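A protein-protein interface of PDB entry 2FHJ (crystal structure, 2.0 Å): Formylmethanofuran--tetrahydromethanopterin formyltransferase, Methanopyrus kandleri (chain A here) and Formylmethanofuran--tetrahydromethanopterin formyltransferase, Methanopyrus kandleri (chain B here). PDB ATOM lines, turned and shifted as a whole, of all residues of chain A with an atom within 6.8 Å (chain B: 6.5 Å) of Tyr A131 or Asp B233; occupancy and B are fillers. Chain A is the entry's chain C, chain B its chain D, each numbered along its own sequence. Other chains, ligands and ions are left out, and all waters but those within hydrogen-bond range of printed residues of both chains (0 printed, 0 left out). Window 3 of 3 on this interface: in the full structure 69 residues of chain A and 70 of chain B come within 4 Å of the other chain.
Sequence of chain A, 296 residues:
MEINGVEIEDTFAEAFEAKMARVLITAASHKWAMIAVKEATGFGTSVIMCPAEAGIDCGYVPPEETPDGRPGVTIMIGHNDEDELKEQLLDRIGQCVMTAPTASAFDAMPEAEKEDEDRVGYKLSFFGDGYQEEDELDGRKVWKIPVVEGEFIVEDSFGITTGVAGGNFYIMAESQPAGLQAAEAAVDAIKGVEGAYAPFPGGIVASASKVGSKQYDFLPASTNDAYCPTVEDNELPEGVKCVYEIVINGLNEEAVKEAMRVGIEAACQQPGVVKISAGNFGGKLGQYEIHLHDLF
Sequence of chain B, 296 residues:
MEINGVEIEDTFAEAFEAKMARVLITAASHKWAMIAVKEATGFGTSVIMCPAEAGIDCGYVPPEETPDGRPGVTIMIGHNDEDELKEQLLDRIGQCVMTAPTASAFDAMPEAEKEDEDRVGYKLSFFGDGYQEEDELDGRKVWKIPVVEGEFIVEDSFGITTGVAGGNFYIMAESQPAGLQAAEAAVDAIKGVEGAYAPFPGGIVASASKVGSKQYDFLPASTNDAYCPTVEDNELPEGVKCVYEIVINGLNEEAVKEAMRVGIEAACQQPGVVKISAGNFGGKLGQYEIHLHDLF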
ATOM      1  N   SER A 125     -29.869  11.739  23.744  1.00  0.00           N
ATOM      2  CA  SER A 125     -30.078  13.061  23.155  1.00  0.00           C
ATOM      3  C   SER A 125     -28.855  13.982  23.187  1.00  0.00           C
ATOM      4  O   SER A 125     -28.732  14.861  22.334  1.00  0.00           O
ATOM      5  CB  SER A 125     -31.290  13.774  23.784  1.00  0.00           C
ATOM      6  OG  SER A 125     -31.020  14.331  25.066  1.00  0.00           O
ATOM      7  N   GLY A 128     -26.806  14.824  20.136  1.00  0.00           N
ATOM      8  CA  GLY A 128     -27.205  15.964  19.313  1.00  0.00           C
ATOM      9  C   GLY A 128     -26.393  17.248  19.507  1.00  0.00           C
ATOM     10  O   GLY A 128     -26.570  18.219  18.763  1.00  0.00           O
ATOM     11  N   ASP A 129     -25.514  17.258  20.514  1.00  0.00           N
ATOM     12  CA  ASP A 129     -24.535  18.331  20.713  1.00  0.00           C
ATOM     13  C   ASP A 129     -25.162  19.722  20.752  1.00  0.00           C
ATOM     14  O   ASP A 129     -24.671  20.663  20.112  1.00  0.00           O
ATOM     15  CB  ASP A 129     -23.468  18.299  19.625  1.00  0.00           C
ATOM     16  CG  ASP A 129     -22.215  19.017  20.036  1.00  0.00           C
ATOM     17  OD1 ASP A 129     -22.087  19.354  21.233  1.00  0.00           O
ATOM     18  OD2 ASP A 129     -21.351  19.239  19.161  1.00  0.00           O
ATOM     19  N   GLY A 130     -26.257  19.839  21.493  1.00  0.00           N
ATOM     20  CA  GLY A 130     -26.934  21.105  21.666  1.00  0.00           C
ATOM     21  C   GLY A 130     -28.099  21.289  20.719  1.00  0.00           C
ATOM     22  O   GLY A 130     -28.996  22.078  20.996  1.00  0.00           O
ATOM     23  N   TYR A 131     -28.096  20.573  19.593  1.00  0.00           N
ATOM     24  CA  TYR A 131     -29.172  20.701  18.598  1.00  0.00           C
ATOM     25  C   TYR A 131     -30.409  19.797  18.825  1.00  0.00           C
ATOM     26  O   TYR A 131     -31.376  19.881  18.067  1.00  0.00           O
ATOM     27  CB  TYR A 131     -28.616  20.453  17.184  1.00  0.00           C
ATOM     28  CG  TYR A 131     -27.483  21.374  16.786  1.00  0.00           C
ATOM     29  CD1 TYR A 131     -26.154  20.975  16.933  1.00  0.00           C
ATOM     30  CD2 TYR A 131     -27.736  22.650  16.275  1.00  0.00           C
ATOM     31  CE1 TYR A 131     -25.103  21.810  16.577  1.00  0.00           C
ATOM     32  CE2 TYR A 131     -26.685  23.502  15.911  1.00  0.00           C
ATOM     33  CZ  TYR A 131     -25.369  23.072  16.066  1.00  0.00           C
ATOM     34  OH  TYR A 131     -24.313  23.896  15.717  1.00  0.00           O
ATOM     35  N   GLN A 132     -30.376  18.938  19.847  1.00  0.00           N
ATOM     36  CA  GLN A 132     -31.518  18.061  20.170  1.00  0.00           C
ATOM     37  C   GLN A 132     -32.751  18.862  20.648  1.00  0.00           C
ATOM     38  O   GLN A 132     -32.608  19.830  21.393  1.00  0.00           O
ATOM     39  CB  GLN A 132     -31.115  16.984  21.195  1.00  0.00           C
ATOM     40  CG  GLN A 132     -30.694  17.493  22.587  1.00  0.00           C
ATOM     41  CD  GLN A 132     -29.247  17.843  22.684  1.00  0.00           C
ATOM     42  OE1 GLN A 132     -28.611  18.165  21.683  1.00  0.00           O
ATOM     43  NE2 GLN A 132     -28.706  17.778  23.896  1.00  0.00           N
ATOM     44  N   GLU A 133     -33.943  18.486  20.167  1.00  0.00           N
ATOM     45  CA  GLU A 133     -35.238  19.063  20.598  1.00  0.00           C
ATOM     46  C   GLU A 133     -36.082  18.004  21.312  1.00  0.00           C
ATOM     47  O   GLU A 133     -36.326  16.932  20.752  1.00  0.00           O
ATOM     48  CB  GLU A 133     -36.107  19.523  19.410  1.00  0.00           C
ATOM     49  CG  GLU A 133     -35.603  20.682  18.549  1.00  0.00           C
ATOM     50  CD  GLU A 133     -36.315  20.728  17.183  1.00  0.00           C
ATOM     51  OE1 GLU A 133     -37.518  20.361  17.118  1.00  0.00           O
ATOM     52  OE2 GLU A 133     -35.666  21.117  16.177  1.00  0.00           O
ATOM     53  N   LYS A 144     -35.873  14.466  19.503  1.00  0.00           N
ATOM     54  CA  LYS A 144     -35.523  14.545  18.081  1.00  0.00           C
ATOM     55  C   LYS A 144     -34.043  14.907  17.968  1.00  0.00           C
ATOM     56  O   LYS A 144     -33.675  16.058  18.187  1.00  0.00           O
ATOM     57  CB  LYS A 144     -36.392  15.593  17.387  1.00  0.00           C
ATOM     58  CG  LYS A 144     -37.880  15.381  17.637  1.00  0.00           C
ATOM     59  CD  LYS A 144     -38.767  15.958  16.532  1.00  0.00           C
ATOM     60  CE  LYS A 144     -38.792  17.486  16.568  1.00  0.00           C
ATOM     61  NZ  LYS A 144     -39.854  18.079  15.677  1.00  0.00           N
ATOM     62  N   ILE A 145     -33.213  13.905  17.670  1.00  0.00           N
ATOM     63  CA  ILE A 145     -31.763  14.039  17.643  1.00  0.00           C
ATOM     64  C   ILE A 145     -31.317  14.236  16.199  1.00  0.00           C
ATOM     65  O   ILE A 145     -31.581  13.374  15.346  1.00  0.00           O
ATOM     66  CB  ILE A 145     -31.074  12.798  18.219  1.00  0.00           C
ATOM     67  CG1 ILE A 145     -31.565  12.536  19.650  1.00  0.00           C
ATOM     68  CG2 ILE A 145     -29.540  12.950  18.160  1.00  0.00           C
ATOM     69  CD1 ILE A 145     -30.985  11.283  20.279  1.00  0.00           C
ATOM     70  N   PRO A 146     -30.652  15.374  15.904  1.00  0.00           N
ATOM     71  CA  PRO A 146     -30.201  15.563  14.526  1.00  0.00           C
ATOM     72  C   PRO A 146     -29.062  14.613  14.180  1.00  0.00           C
ATOM     73  O   PRO A 146     -28.080  14.490  14.921  1.00  0.00           O
ATOM     74  CB  PRO A 146     -29.753  17.031  14.467  1.00  0.00           C
ATOM     75  CG  PRO A 146     -29.812  17.553  15.829  1.00  0.00           C
ATOM     76  CD  PRO A 146     -30.269  16.495  16.780  1.00  0.00           C
ATOM     77  N   GLU A 151     -33.238  12.921  11.254  1.00  0.00           N
ATOM     78  CA  GLU A 151     -33.433  12.893  12.725  1.00  0.00           C
ATOM     79  C   GLU A 151     -33.546  11.480  13.275  1.00  0.00           C
ATOM     80  O   GLU A 151     -34.065  10.589  12.604  1.00  0.00           O
ATOM     81  CB  GLU A 151     -34.692  13.653  13.104  1.00  0.00           C
ATOM     82  CG  GLU A 151     -34.480  15.137  13.170  1.00  0.00           C
ATOM     83  CD  GLU A 151     -35.773  15.894  13.393  1.00  0.00           C
ATOM     84  OE1 GLU A 151     -36.857  15.305  13.130  1.00  0.00           O
ATOM     85  OE2 GLU A 151     -35.695  17.074  13.833  1.00  0.00           O
ATOM     86  N   LYS B 210     -19.057  13.217  14.846  1.00  0.00           N
ATOM     87  CA  LYS B 210     -17.823  13.998  14.800  1.00  0.00           C
ATOM     88  C   LYS B 210     -17.117  13.802  16.122  1.00  0.00           C
ATOM     89  O   LYS B 210     -17.753  13.427  17.107  1.00  0.00           O
ATOM     90  CB  LYS B 210     -18.121  15.482  14.598  1.00  0.00           C
ATOM     91  CG  LYS B 210     -18.777  16.173  15.800  1.00  0.00           C
ATOM     92  CD  LYS B 210     -19.037  17.639  15.544  1.00  0.00           C
ATOM     93  CE  LYS B 210     -19.704  18.328  16.723  1.00  0.00           C
ATOM     94  NZ  LYS B 210     -21.182  18.129  16.781  1.00  0.00           N
ATOM     95  N   LYS B 214     -19.427  20.487  20.629  1.00  0.00           N
ATOM     96  CA  LYS B 214     -19.330  21.934  20.713  1.00  0.00           C
ATOM     97  C   LYS B 214     -19.989  22.505  21.969  1.00  0.00           C
ATOM     98  O   LYS B 214     -19.530  23.524  22.480  1.00  0.00           O
ATOM     99  CB  LYS B 214     -19.887  22.569  19.432  1.00  0.00           C
ATOM    100  CG  LYS B 214     -19.059  22.131  18.201  1.00  0.00           C
ATOM    101  CD  LYS B 214     -19.272  22.992  16.975  1.00  0.00           C
ATOM    102  CE  LYS B 214     -20.669  22.842  16.421  1.00  0.00           C
ATOM    103  NZ  LYS B 214     -21.082  21.423  16.397  1.00  0.00           N
ATOM    104  N   GLN B 215     -21.033  21.840  22.473  1.00  0.00           N
ATOM    105  CA  GLN B 215     -21.724  22.281  23.690  1.00  0.00           C
ATOM    106  C   GLN B 215     -21.368  21.484  24.944  1.00  0.00           C
ATOM    107  O   GLN B 215     -21.361  22.057  26.036  1.00  0.00           O
ATOM    108  CB  GLN B 215     -23.246  22.303  23.495  1.00  0.00           C
ATOM    109  CG  GLN B 215     -23.746  23.485  22.642  1.00  0.00           C
ATOM    110  CD  GLN B 215     -25.044  24.098  23.160  1.00  0.00           C
ATOM    111  OE1 GLN B 215     -25.173  24.380  24.351  1.00  0.00           O
ATOM    112  NE2 GLN B 215     -26.001  24.328  22.259  1.00  0.00           N
ATOM    113  N   TYR B 216     -21.076  20.187  24.811  1.00  0.00           N
ATOM    114  CA  TYR B 216     -20.859  19.334  25.988  1.00  0.00           C
ATOM    115  C   TYR B 216     -19.407  18.963  26.126  1.00  0.00           C
ATOM    116  O   TYR B 216     -18.894  18.175  25.349  1.00  0.00           O
ATOM    117  CB  TYR B 216     -21.742  18.075  25.938  1.00  0.00           C
ATOM    118  CG  TYR B 216     -23.171  18.437  25.660  1.00  0.00           C
ATOM    119  CD1 TYR B 216     -23.792  18.037  24.497  1.00  0.00           C
ATOM    120  CD2 TYR B 216     -23.876  19.256  26.528  1.00  0.00           C
ATOM    121  CE1 TYR B 216     -25.080  18.428  24.218  1.00  0.00           C
ATOM    122  CE2 TYR B 216     -25.178  19.640  26.259  1.00  0.00           C
ATOM    123  CZ  TYR B 216     -25.765  19.228  25.090  1.00  0.00           C
ATOM    124  OH  TYR B 216     -27.056  19.609  24.812  1.00  0.00           O
ATOM    125  N   THR B 223     -23.173  14.081  17.183  1.00  0.00           N
ATOM    126  CA  THR B 223     -23.651  14.103  15.828  1.00  0.00           C
ATOM    127  C   THR B 223     -22.752  15.007  14.963  1.00  0.00           C
ATOM    128  O   THR B 223     -22.319  16.095  15.383  1.00  0.00           O
ATOM    129  CB  THR B 223     -25.131  14.511  15.746  1.00  0.00           C
ATOM    130  OG1 THR B 223     -25.656  14.101  14.479  1.00  0.00           O
ATOM    131  CG2 THR B 223     -25.338  16.025  15.946  1.00  0.00           C
ATOM    132  N   ASP B 225     -22.672  17.486  13.010  1.00  0.00           N
ATOM    133  CA  ASP B 225     -23.616  18.559  12.715  1.00  0.00           C
ATOM    134  C   ASP B 225     -23.247  19.221  11.412  1.00  0.00           C
ATOM    135  O   ASP B 225     -24.126  19.779  10.755  1.00  0.00           O
ATOM    136  CB  ASP B 225     -23.748  19.592  13.845  1.00  0.00           C
ATOM    137  CG  ASP B 225     -22.438  20.282  14.185  1.00  0.00           C
ATOM    138  OD1 ASP B 225     -21.489  19.568  14.556  1.00  0.00           O
ATOM    139  OD2 ASP B 225     -22.373  21.538  14.122  1.00  0.00           O
ATOM    140  N   ALA B 226     -21.969  19.113  11.024  1.00  0.00           N
ATOM    141  CA  ALA B 226     -21.519  19.634   9.738  1.00  0.00           C
ATOM    142  C   ALA B 226     -22.265  18.969   8.580  1.00  0.00           C
ATOM    143  O   ALA B 226     -22.570  19.636   7.605  1.00  0.00           O
ATOM    144  CB  ALA B 226     -20.021  19.486   9.570  1.00  0.00           C
ATOM    145  N   CYS B 228     -25.362  17.324   9.147  1.00  0.00           N
ATOM    146  CA  CYS B 228     -26.764  17.196   9.557  1.00  0.00           C
ATOM    147  C   CYS B 228     -27.684  18.133   8.765  1.00  0.00           C
ATOM    148  O   CYS B 228     -27.584  19.350   8.882  1.00  0.00           O
ATOM    149  CB  CYS B 228     -26.912  17.483  11.052  1.00  0.00           C
ATOM    150  SG  CYS B 228     -26.420  16.153  12.067  1.00  0.00           S
ATOM    151  N   THR B 230     -30.767  19.029   9.158  1.00  0.00           N
ATOM    152  CA  THR B 230     -31.683  19.834   9.970  1.00  0.00           C
ATOM    153  C   THR B 230     -30.984  20.843  10.863  1.00  0.00           C
ATOM    154  O   THR B 230     -31.645  21.611  11.565  1.00  0.00           O
ATOM    155  CB  THR B 230     -32.575  18.967  10.863  1.00  0.00           C
ATOM    156  OG1 THR B 230     -31.760  18.257  11.801  1.00  0.00           O
ATOM    157  CG2 THR B 230     -33.375  17.988  10.021  1.00  0.00           C
ATOM    158  N   VAL B 231     -29.665  20.859  10.840  1.00  0.00           N
ATOM    159  CA  VAL B 231     -28.951  21.936  11.479  1.00  0.00           C
ATOM    160  C   VAL B 231     -28.821  23.084  10.463  1.00  0.00           C
ATOM    161  O   VAL B 231     -28.336  22.877   9.348  1.00  0.00           O
ATOM    162  CB  VAL B 231     -27.611  21.460  11.989  1.00  0.00           C
ATOM    163  CG1 VAL B 231     -26.862  22.607  12.625  1.00  0.00           C
ATOM    164  CG2 VAL B 231     -27.830  20.331  12.990  1.00  0.00           C
ATOM    165  N   GLU B 232     -29.296  24.272  10.849  1.00  0.00           N
ATOM    166  CA  GLU B 232     -29.246  25.464   9.996  1.00  0.00           C
ATOM    167  C   GLU B 232     -27.814  25.829   9.561  1.00  0.00           C
ATOM    168  O   GLU B 232     -27.602  26.263   8.423  1.00  0.00           O
ATOM    169  N   ASP B 233     -26.849  25.632  10.466  1.00  0.00           N
ATOM    170  CA  ASP B 233     -25.430  25.961  10.215  1.00  0.00           C
ATOM    171  C   ASP B 233     -24.570  24.757   9.770  1.00  0.00           C
ATOM    172  O   ASP B 233     -23.485  24.532  10.311  1.00  0.00           O
ATOM    173  CB  ASP B 233     -24.793  26.570  11.479  1.00  0.00           C
ATOM    174  CG  ASP B 233     -25.130  25.706  12.704  1.00  0.00           C
ATOM    175  OD1 ASP B 233     -24.207  25.104  13.301  1.00  0.00           O
ATOM    176  OD2 ASP B 233     -26.335  25.596  13.035  1.00  0.00           O
ATOM    177  N   ASN B 234     -25.032  24.005   8.776  1.00  0.00           N
ATOM    178  CA  ASN B 234     -24.298  22.833   8.287  1.00  0.00           C
ATOM    179  C   ASN B 234     -23.377  23.170   7.099  1.00  0.00           C
ATOM    180  O   ASN B 234     -23.519  24.217   6.493  1.00  0.00           O
ATOM    181  CB  ASN B 234     -25.275  21.708   7.937  1.00  0.00           C
ATOM    182  CG  ASN B 234     -26.171  22.045   6.768  1.00  0.00           C
ATOM    183  OD1 ASN B 234     -27.247  21.474   6.618  1.00  0.00           O
ATOM    184  ND2 ASN B 234     -25.731  22.966   5.926  1.00  0.00           N
ATOM    185  N   GLU B 235     -22.442  22.270   6.788  1.00  0.00           N
ATOM    186  CA  GLU B 235     -21.513  22.413   5.664  1.00  0.00           C
ATOM    187  C   GLU B 235     -21.960  21.566   4.454  1.00  0.00           C
ATOM    188  O   GLU B 235     -21.131  21.032   3.719  1.00  0.00           O
ATOM    189  CB  GLU B 235     -20.093  21.984   6.090  1.00  0.00           C
ATOM    190  CG  GLU B 235     -19.498  22.777   7.245  1.00  0.00           C
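Of the 14 printed residues of chain B, 10 touch a printed residue of chain A.
Hydrophobic or aromatic side chains of chain B that line the printed part of chain A: Tyr B216 and Val B231.
Printed residues of chain A that touch a printed residue of chain B: Gly A128, Asp A129, Gly A130, Tyr A131, Gln A132 and Pro A146.
Among the printed residues, Asp or Glu carboxylates within 4 Å of a Lys or Arg side-chain nitrogen of the other chain: Asp A129 with Lys B210 and Asp A129 with Lys B214.
Gly A128 touches Thr B223.
Asp A129 touches Tyr B216.
Gly A130 touches Gln B215.
Tyr A131 touches Lys B214 (OH to CE, 3.9 Å).
CE2 of Tyr A131 touches CG1 of Val B231 (3.4 Å).
Pro A146 touches Thr B230 (CB to OG1, 3.6 Å).
O of Ser A125 sits close to NE2 of Gln A132 (3.3 Å).
The backbone NH of Asp A129 lies within hydrogen-bond range of the side-chain amide oxygen of Gln A132 (3.4 Å).
The backbone NH (N) of Gly A130 lies within hydrogen-bond range of the side-chain amide oxygen (OE1) of Gln A132, at 2.9 Å.
NZ of Lys B210 lies within salt-bridge range of OD1 of Asp B225, at 2.7 Å.
NZ of Lys B214 lies within salt-bridge range of OD2 of Asp B225, 2.6 Å away.
The side-chain amide oxygen of Asn B234 sits close to the backbone carbonyl oxygen of Val B231 (3.3 Å).
Of the printed residues of chain B, Gly A130 touches Gln B215 and Tyr B216.
Of the printed residues of chain B, Tyr A131 touches Lys B214 (3.9 Å), Asp B225 (3.4 Å), Val B231 (3.4 Å) and Asp B233 (2.7 Å).
Printed residues of chain A within 4 Å of Lys B210: Asp A129 (2.6 Å).
Printed residues of chain A within 4 Å of Lys B214: Asp A129 and Tyr A131.
Printed residues of chain A within 4 Å of Thr B223: Gly A128 and Pro A146.
Of the printed residues of chain A, Asp B233 touches Tyr A131 (2.7 Å).
The nearest printed residue of chain B that does not touch Tyr A131 is Gln B215 (5.1 Å).
The nearest printed residue of chain A that does not touch Asp B233 is Asp A129 (8.1 Å).
The side-chain amino group (NZ) of Lys B210 is in salt-bridge range of the side-chain carboxylate (OD2) of Asp A129 (2.6 Å).
The side-chain amino group (NZ) of Lys B214 lies within salt-bridge range of the side-chain carboxylate (OD2) of Asp A129, at 3.5 Å.
N of Gln B215 lies within hydrogen-bond range of OD1 of Asp A129, 3.0 Å away.
The backbone NH (N) of Gly A130 sits close to the side-chain hydroxyl (OH) of Tyr B216, at 3.4 Å.
The side-chain carboxylate (OD2) of Asp B225 is in hydrogen-bond range of the side-chain hydroxyl (OH) of Tyr A131, 3.4 Å away.
The side-chain hydroxyl (OH) of Tyr A131 lies within hydrogen-bond range of the side-chain carboxylate (OD1) of Asp B233 (2.7 Å).
NE2 of Gln A132 is in hydrogen-bond range of OH of Tyr B216, 2.6 Å away.
The side-chain hydroxyl (OG1) of Thr B223 is in hydrogen-bond range of the backbone carbonyl oxygen (O) of Pro A146.
O of Pro A146 lies within hydrogen-bond range of SG of Cys B228 (3.7 Å).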
